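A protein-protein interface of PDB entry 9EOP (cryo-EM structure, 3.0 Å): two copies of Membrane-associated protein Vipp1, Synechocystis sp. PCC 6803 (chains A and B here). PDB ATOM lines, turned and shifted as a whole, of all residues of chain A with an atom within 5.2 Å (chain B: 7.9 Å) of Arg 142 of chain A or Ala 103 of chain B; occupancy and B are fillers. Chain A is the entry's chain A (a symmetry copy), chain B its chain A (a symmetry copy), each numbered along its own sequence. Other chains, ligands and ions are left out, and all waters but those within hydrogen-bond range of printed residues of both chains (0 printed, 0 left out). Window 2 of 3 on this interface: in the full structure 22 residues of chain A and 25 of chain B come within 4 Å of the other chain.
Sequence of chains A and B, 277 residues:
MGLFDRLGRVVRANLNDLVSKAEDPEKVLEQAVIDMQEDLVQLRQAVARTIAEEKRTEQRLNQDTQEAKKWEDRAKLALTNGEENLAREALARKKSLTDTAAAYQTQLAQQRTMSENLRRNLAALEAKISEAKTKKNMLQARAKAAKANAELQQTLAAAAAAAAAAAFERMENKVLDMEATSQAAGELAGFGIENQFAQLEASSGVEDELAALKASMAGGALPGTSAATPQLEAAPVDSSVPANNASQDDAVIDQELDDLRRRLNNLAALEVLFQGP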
ATOM      1  N   MET A 138       6.693  19.436   9.479  1.00  0.00           N
ATOM      2  CA  MET A 138       7.182  19.405  10.852  1.00  0.00           C
ATOM      3  C   MET A 138       7.844  18.083  11.211  1.00  0.00           C
ATOM      4  O   MET A 138       8.806  18.055  11.985  1.00  0.00           O
ATOM      5  CB  MET A 138       6.026  19.656  11.804  1.00  0.00           C
ATOM      6  CG  MET A 138       6.406  19.576  13.254  1.00  0.00           C
ATOM      7  SD  MET A 138       6.053  17.970  13.982  1.00  0.00           S
ATOM      8  CE  MET A 138       4.273  17.986  13.968  1.00  0.00           C
ATOM      9  N   LEU A 139       7.341  16.982  10.673  1.00  0.00           N
ATOM     10  CA  LEU A 139       7.934  15.676  10.914  1.00  0.00           C
ATOM     11  C   LEU A 139       9.239  15.450  10.167  1.00  0.00           C
ATOM     12  O   LEU A 139      10.159  14.831  10.706  1.00  0.00           O
ATOM     13  CB  LEU A 139       6.937  14.598  10.525  1.00  0.00           C
ATOM     14  CG  LEU A 139       5.674  14.504  11.368  1.00  0.00           C
ATOM     15  CD1 LEU A 139       4.808  13.434  10.809  1.00  0.00           C
ATOM     16  CD2 LEU A 139       5.973  14.224  12.814  1.00  0.00           C
ATOM     17  N   GLN A 140       9.348  15.936   8.938  1.00  0.00           N
ATOM     18  CA  GLN A 140      10.615  15.837   8.234  1.00  0.00           C
ATOM     19  C   GLN A 140      11.691  16.709   8.861  1.00  0.00           C
ATOM     20  O   GLN A 140      12.869  16.341   8.853  1.00  0.00           O
ATOM     21  CB  GLN A 140      10.400  16.236   6.785  1.00  0.00           C
ATOM     22  CG  GLN A 140       9.690  15.193   5.983  1.00  0.00           C
ATOM     23  CD  GLN A 140       9.436  15.618   4.565  1.00  0.00           C
ATOM     24  OE1 GLN A 140       9.132  16.776   4.295  1.00  0.00           O
ATOM     25  NE2 GLN A 140       9.526  14.672   3.649  1.00  0.00           N
ATOM     26  N   ALA A 141      11.309  17.860   9.398  1.00  0.00           N
ATOM     27  CA  ALA A 141      12.226  18.677  10.179  1.00  0.00           C
ATOM     28  C   ALA A 141      12.787  17.934  11.383  1.00  0.00           C
ATOM     29  O   ALA A 141      14.001  17.910  11.609  1.00  0.00           O
ATOM     30  CB  ALA A 141      11.501  19.930  10.643  1.00  0.00           C
ATOM     31  N   ARG A 142      11.906  17.321  12.163  1.00  0.00           N
ATOM     32  CA  ARG A 142      12.309  16.548  13.330  1.00  0.00           C
ATOM     33  C   ARG A 142      13.173  15.347  12.979  1.00  0.00           C
ATOM     34  O   ARG A 142      14.075  14.983  13.740  1.00  0.00           O
ATOM     35  CB  ARG A 142      11.047  16.106  14.045  1.00  0.00           C
ATOM     36  CG  ARG A 142      10.412  17.190  14.848  1.00  0.00           C
ATOM     37  CD  ARG A 142       9.173  16.715  15.543  1.00  0.00           C
ATOM     38  NE  ARG A 142       8.704  17.683  16.518  1.00  0.00           N
ATOM     39  CZ  ARG A 142       7.901  17.390  17.530  1.00  0.00           C
ATOM     40  NH1 ARG A 142       7.456  16.162  17.722  1.00  0.00           N
ATOM     41  NH2 ARG A 142       7.551  18.351  18.380  1.00  0.00           N
ATOM     42  N   ALA A 143      12.905  14.707  11.850  1.00  0.00           N
ATOM     43  CA  ALA A 143      13.699  13.556  11.443  1.00  0.00           C
ATOM     44  C   ALA A 143      15.130  13.930  11.079  1.00  0.00           C
ATOM     45  O   ALA A 143      16.062  13.162  11.341  1.00  0.00           O
ATOM     46  CB  ALA A 143      13.025  12.862  10.272  1.00  0.00           C
ATOM     47  N   LYS A 144      15.325  15.093  10.469  1.00  0.00           N
ATOM     48  CA  LYS A 144      16.670  15.570  10.170  1.00  0.00           C
ATOM     49  C   LYS A 144      17.442  15.973  11.417  1.00  0.00           C
ATOM     50  O   LYS A 144      18.628  15.653  11.548  1.00  0.00           O
ATOM     51  CB  LYS A 144      16.585  16.743   9.207  1.00  0.00           C
ATOM     52  CG  LYS A 144      16.187  16.348   7.809  1.00  0.00           C
ATOM     53  CD  LYS A 144      15.896  17.551   6.933  1.00  0.00           C
ATOM     54  CE  LYS A 144      17.107  18.462   6.790  1.00  0.00           C
ATOM     55  NZ  LYS A 144      18.197  17.826   6.005  1.00  0.00           N
ATOM     56  N   ALA A 145      16.798  16.678  12.339  1.00  0.00           N
ATOM     57  CA  ALA A 145      17.455  17.047  13.585  1.00  0.00           C
ATOM     58  C   ALA A 145      17.862  15.831  14.402  1.00  0.00           C
ATOM     59  O   ALA A 145      18.991  15.749  14.893  1.00  0.00           O
ATOM     60  CB  ALA A 145      16.533  17.945  14.393  1.00  0.00           C
ATOM     61  N   ALA A 146      16.953  14.879  14.568  1.00  0.00           N
ATOM     62  CA  ALA A 146      17.263  13.690  15.348  1.00  0.00           C
ATOM     63  C   ALA A 146      18.477  12.954  14.806  1.00  0.00           C
ATOM     64  O   ALA A 146      19.294  12.434  15.572  1.00  0.00           O
ATOM     65  CB  ALA A 146      16.057  12.766  15.351  1.00  0.00           C
ATOM     66  N   LYS A 147      18.608  12.904  13.491  1.00  0.00           N
ATOM     67  CA  LYS A 147      19.697  12.188  12.846  1.00  0.00           C
ATOM     68  C   LYS A 147      21.029  12.917  12.927  1.00  0.00           C
ATOM     69  O   LYS A 147      22.083  12.273  12.930  1.00  0.00           O
ATOM     70  CB  LYS A 147      19.304  11.932  11.402  1.00  0.00           C
ATOM     71  CG  LYS A 147      20.232  11.066  10.628  1.00  0.00           C
ATOM     72  CD  LYS A 147      19.474  10.354   9.515  1.00  0.00           C
ATOM     73  CE  LYS A 147      18.604  11.297   8.697  1.00  0.00           C
ATOM     74  NZ  LYS A 147      17.783  10.558   7.707  1.00  0.00           N
ATOM     75  N   GLU B  53      20.426  23.788  11.829  1.00  0.00           N
ATOM     76  CA  GLU B  53      19.012  23.493  11.952  1.00  0.00           C
ATOM     77  C   GLU B  53      18.313  24.266  13.055  1.00  0.00           C
ATOM     78  O   GLU B  53      17.088  24.397  13.013  1.00  0.00           O
ATOM     79  CB  GLU B  53      18.840  21.994  12.187  1.00  0.00           C
ATOM     80  CG  GLU B  53      19.494  21.212  11.086  1.00  0.00           C
ATOM     81  CD  GLU B  53      19.002  19.805  10.982  1.00  0.00           C
ATOM     82  OE1 GLU B  53      18.821  19.174  12.036  1.00  0.00           O
ATOM     83  OE2 GLU B  53      18.801  19.329   9.847  1.00  0.00           O
ATOM     84  N   THR B  57      14.722  25.950  12.015  1.00  0.00           N
ATOM     85  CA  THR B  57      13.417  25.915  12.670  1.00  0.00           C
ATOM     86  C   THR B  57      12.880  27.306  12.969  1.00  0.00           C
ATOM     87  O   THR B  57      11.664  27.493  13.062  1.00  0.00           O
ATOM     88  CB  THR B  57      13.502  25.118  13.963  1.00  0.00           C
ATOM     89  OG1 THR B  57      14.481  25.701  14.822  1.00  0.00           O
ATOM     90  CG2 THR B  57      13.892  23.705  13.671  1.00  0.00           C
ATOM     91  N   ARG B  60      11.018  28.341   9.732  1.00  0.00           N
ATOM     92  CA  ARG B  60       9.733  27.662   9.637  1.00  0.00           C
ATOM     93  C   ARG B  60       8.696  28.241  10.589  1.00  0.00           C
ATOM     94  O   ARG B  60       7.531  28.424  10.220  1.00  0.00           O
ATOM     95  CB  ARG B  60       9.934  26.189   9.935  1.00  0.00           C
ATOM     96  CG  ARG B  60      10.896  25.496   9.023  1.00  0.00           C
ATOM     97  CD  ARG B  60      10.998  24.048   9.389  1.00  0.00           C
ATOM     98  NE  ARG B  60      12.234  23.433   8.934  1.00  0.00           N
ATOM     99  CZ  ARG B  60      12.389  22.831   7.767  1.00  0.00           C
ATOM    100  NH1 ARG B  60      11.436  22.842   6.850  1.00  0.00           N
ATOM    101  NH2 ARG B  60      13.534  22.208   7.510  1.00  0.00           N
ATOM    102  N   LEU B  61       9.105  28.522  11.820  1.00  0.00           N
ATOM    103  CA  LEU B  61       8.215  29.122  12.806  1.00  0.00           C
ATOM    104  C   LEU B  61       7.634  30.453  12.347  1.00  0.00           C
ATOM    105  O   LEU B  61       6.451  30.728  12.571  1.00  0.00           O
ATOM    106  CB  LEU B  61       8.981  29.293  14.109  1.00  0.00           C
ATOM    107  CG  LEU B  61       8.325  30.078  15.225  1.00  0.00           C
ATOM    108  CD1 LEU B  61       7.049  29.428  15.614  1.00  0.00           C
ATOM    109  CD2 LEU B  61       9.255  30.115  16.386  1.00  0.00           C
ATOM    110  N   LEU B  97      -2.076  24.777  12.062  1.00  0.00           N
ATOM    111  CA  LEU B  97      -0.903  25.643  12.019  1.00  0.00           C
ATOM    112  C   LEU B  97      -0.445  26.085  13.404  1.00  0.00           C
ATOM    113  O   LEU B  97       0.756  26.096  13.691  1.00  0.00           O
ATOM    114  CB  LEU B  97      -1.210  26.858  11.158  1.00  0.00           C
ATOM    115  CG  LEU B  97      -1.354  26.557   9.674  1.00  0.00           C
ATOM    116  CD1 LEU B  97      -2.067  27.665   8.974  1.00  0.00           C
ATOM    117  CD2 LEU B  97      -0.005  26.368   9.069  1.00  0.00           C
ATOM    118  N   THR B  98      -1.379  26.464  14.268  1.00  0.00           N
ATOM    119  CA  THR B  98      -1.033  26.811  15.643  1.00  0.00           C
ATOM    120  C   THR B  98      -0.507  25.621  16.429  1.00  0.00           C
ATOM    121  O   THR B  98       0.380  25.777  17.277  1.00  0.00           O
ATOM    122  CB  THR B  98      -2.246  27.385  16.358  1.00  0.00           C
ATOM    123  OG1 THR B  98      -3.238  26.363  16.494  1.00  0.00           O
ATOM    124  CG2 THR B  98      -2.822  28.531  15.586  1.00  0.00           C
ATOM    125  N   ASP B  99      -1.038  24.430  16.179  1.00  0.00           N
ATOM    126  CA  ASP B  99      -0.530  23.249  16.863  1.00  0.00           C
ATOM    127  C   ASP B  99       0.903  22.913  16.476  1.00  0.00           C
ATOM    128  O   ASP B  99       1.719  22.587  17.344  1.00  0.00           O
ATOM    129  CB  ASP B  99      -1.433  22.061  16.561  1.00  0.00           C
ATOM    130  CG  ASP B  99      -2.767  22.145  17.269  1.00  0.00           C
ATOM    131  OD1 ASP B  99      -2.889  22.948  18.218  1.00  0.00           O
ATOM    132  OD2 ASP B  99      -3.693  21.406  16.878  1.00  0.00           O
ATOM    133  N   THR B 100       1.236  22.983  15.191  1.00  0.00           N
ATOM    134  CA  THR B 100       2.607  22.685  14.790  1.00  0.00           C
ATOM    135  C   THR B 100       3.587  23.799  15.136  1.00  0.00           C
ATOM    136  O   THR B 100       4.776  23.529  15.322  1.00  0.00           O
ATOM    137  CB  THR B 100       2.651  22.384  13.296  1.00  0.00           C
ATOM    138  OG1 THR B 100       3.886  21.742  12.979  1.00  0.00           O
ATOM    139  CG2 THR B 100       2.534  23.638  12.498  1.00  0.00           C
ATOM    140  N   ALA B 101       3.123  25.044  15.225  1.00  0.00           N
ATOM    141  CA  ALA B 101       4.001  26.123  15.667  1.00  0.00           C
ATOM    142  C   ALA B 101       4.473  25.948  17.101  1.00  0.00           C
ATOM    143  O   ALA B 101       5.593  26.344  17.440  1.00  0.00           O
ATOM    144  CB  ALA B 101       3.285  27.456  15.521  1.00  0.00           C
ATOM    145  N   ALA B 102       3.637  25.371  17.957  1.00  0.00           N
ATOM    146  CA  ALA B 102       4.040  25.066  19.322  1.00  0.00           C
ATOM    147  C   ALA B 102       5.124  24.001  19.382  1.00  0.00           C
ATOM    148  O   ALA B 102       5.926  23.982  20.319  1.00  0.00           O
ATOM    149  CB  ALA B 102       2.825  24.626  20.121  1.00  0.00           C
ATOM    150  N   ALA B 103       5.154  23.108  18.398  1.00  0.00           N
ATOM    151  CA  ALA B 103       6.216  22.117  18.301  1.00  0.00           C
ATOM    152  C   ALA B 103       7.562  22.736  17.956  1.00  0.00           C
ATOM    153  O   ALA B 103       8.599  22.299  18.465  1.00  0.00           O
ATOM    154  CB  ALA B 103       5.843  21.073  17.260  1.00  0.00           C
ATOM    155  N   TYR B 104       7.575  23.749  17.097  1.00  0.00           N
ATOM    156  CA  TYR B 104       8.820  24.444  16.803  1.00  0.00           C
ATOM    157  C   TYR B 104       9.356  25.223  17.997  1.00  0.00           C
ATOM    158  O   TYR B 104      10.565  25.218  18.248  1.00  0.00           O
ATOM    159  CB  TYR B 104       8.614  25.387  15.626  1.00  0.00           C
ATOM    160  CG  TYR B 104       8.305  24.722  14.312  1.00  0.00           C
ATOM    161  CD1 TYR B 104       9.123  23.735  13.807  1.00  0.00           C
ATOM    162  CD2 TYR B 104       7.224  25.118  13.552  1.00  0.00           C
ATOM    163  CE1 TYR B 104       8.853  23.139  12.606  1.00  0.00           C
ATOM    164  CE2 TYR B 104       6.955  24.535  12.348  1.00  0.00           C
ATOM    165  CZ  TYR B 104       7.769  23.548  11.879  1.00  0.00           C
ATOM    166  OH  TYR B 104       7.492  22.977  10.667  1.00  0.00           O
ATOM    167  N   GLN B 105       8.490  25.906  18.740  1.00  0.00           N
ATOM    168  CA  GLN B 105       8.948  26.587  19.947  1.00  0.00           C
ATOM    169  C   GLN B 105       9.597  25.632  20.937  1.00  0.00           C
ATOM    170  O   GLN B 105      10.624  25.955  21.543  1.00  0.00           O
ATOM    171  CB  GLN B 105       7.782  27.303  20.610  1.00  0.00           C
ATOM    172  CG  GLN B 105       7.423  28.591  19.952  1.00  0.00           C
ATOM    173  CD  GLN B 105       8.364  29.706  20.328  1.00  0.00           C
ATOM    174  OE1 GLN B 105       9.437  29.468  20.881  1.00  0.00           O
ATOM    175  NE2 GLN B 105       7.970  30.934  20.029  1.00  0.00           N
ATOM    176  N   THR B 106       9.012  24.455  21.119  1.00  0.00           N
ATOM    177  CA  THR B 106       9.590  23.461  22.014  1.00  0.00           C
ATOM    178  C   THR B 106      10.913  22.927  21.485  1.00  0.00           C
ATOM    179  O   THR B 106      11.897  22.816  22.224  1.00  0.00           O
ATOM    180  CB  THR B 106       8.595  22.324  22.208  1.00  0.00           C
ATOM    181  OG1 THR B 106       7.364  22.850  22.714  1.00  0.00           O
ATOM    182  CG2 THR B 106       9.128  21.307  23.170  1.00  0.00           C
ATOM    183  N   GLN B 107      10.945  22.592  20.201  1.00  0.00           N
ATOM    184  CA  GLN B 107      12.160  22.119  19.553  1.00  0.00           C
ATOM    185  C   GLN B 107      13.268  23.163  19.598  1.00  0.00           C
ATOM    186  O   GLN B 107      14.407  22.865  19.968  1.00  0.00           O
ATOM    187  CB  GLN B 107      11.820  21.740  18.114  1.00  0.00           C
ATOM    188  CG  GLN B 107      12.943  21.215  17.275  1.00  0.00           C
ATOM    189  CD  GLN B 107      13.288  19.788  17.612  1.00  0.00           C
ATOM    190  OE1 GLN B 107      12.989  19.302  18.700  1.00  0.00           O
ATOM    191  NE2 GLN B 107      13.898  19.094  16.663  1.00  0.00           N
ATOM    192  N   LEU B 108      12.946  24.397  19.225  1.00  0.00           N
ATOM    193  CA  LEU B 108      13.940  25.463  19.150  1.00  0.00           C
ATOM    194  C   LEU B 108      14.550  25.795  20.506  1.00  0.00           C
ATOM    195  O   LEU B 108      15.770  25.939  20.631  1.00  0.00           O
ATOM    196  CB  LEU B 108      13.285  26.698  18.552  1.00  0.00           C
ATOM    197  CG  LEU B 108      14.129  27.955  18.448  1.00  0.00           C
ATOM    198  CD1 LEU B 108      15.271  27.725  17.509  1.00  0.00           C
ATOM    199  CD2 LEU B 108      13.275  29.085  17.969  1.00  0.00           C
ATOM    200  N   ALA B 109      13.719  25.925  21.534  1.00  0.00           N
ATOM    201  CA  ALA B 109      14.228  26.238  22.865  1.00  0.00           C
ATOM    202  C   ALA B 109      15.175  25.167  23.381  1.00  0.00           C
ATOM    203  O   ALA B 109      16.145  25.470  24.084  1.00  0.00           O
ATOM    204  CB  ALA B 109      13.065  26.414  23.830  1.00  0.00           C
ATOM    205  N   GLN B 111      17.027  23.079  21.330  1.00  0.00           N
ATOM    206  CA  GLN B 111      18.218  23.080  20.488  1.00  0.00           C
ATOM    207  C   GLN B 111      19.249  24.115  20.921  1.00  0.00           C
ATOM    208  O   GLN B 111      20.437  23.802  21.049  1.00  0.00           O
ATOM    209  CB  GLN B 111      17.784  23.356  19.057  1.00  0.00           C
ATOM    210  CG  GLN B 111      17.233  22.162  18.343  1.00  0.00           C
ATOM    211  CD  GLN B 111      16.783  22.480  16.940  1.00  0.00           C
ATOM    212  OE1 GLN B 111      16.115  23.481  16.704  1.00  0.00           O
ATOM    213  NE2 GLN B 111      17.126  21.619  16.004  1.00  0.00           N
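N of Ala 145 of chain A lies close to OE1 of Glu 53 of chain B.
The side-chain hydroxyl (OG1) of Thr 57 of chain B sits close to the backbone carbonyl oxygen (O) of Glu 53 of chain B (3.4 Å). The guanidinium group of Arg 142 of chain A is in hydrogen-bond range of the side-chain sulfur of Met 138 of chain A (3.7 Å).
Among the printed residues, pairs that only touch across the chains: Met 138 of chain A with Thr 100 of chain B (3.2 Å), Arg 142 of chain A with Ala 103 of chain B (3.4 Å), Lys 144 of chain A with Glu 53 of chain B (3.5 Å), Met 138 of chain A with Tyr 104 of chain B (3.6 Å), Ala 145 of chain A with Gln 107 of chain B (3.7 Å) and Ala 141 of chain A with Arg 60 of chain B (3.97 Å).
Arg 142 of chain A touches just one residue of chain B: Ala 103. Ala 103 of chain B touches one residue of chain A. No residue of chain B comes within 4 Å of Ala 143 of chain A. Of the printed residues of chain B, Met 138 of chain A touches Thr 100 and Tyr 104. Printed residues of chain A within 4 Å of Glu 53 of chain B: Lys 144 (3.5 Å) and Ala 145 (3.0 Å). The nearest residue of chain B that does not touch Arg 142 of chain A is Gln 107 of chain B (4.4 Å).
Of the 10 printed residues of chain A, 5 touch a printed residue of chain B. Along chain A the printed residues that touch a printed residue of chain B span positions 138 to 145. Hydrophobic or aromatic side chains of chain B that line the printed part of chain A: Ala 103 and Tyr 104. Among the printed residues, 7 pairs touch across the chains.
No position is printed for both chains.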
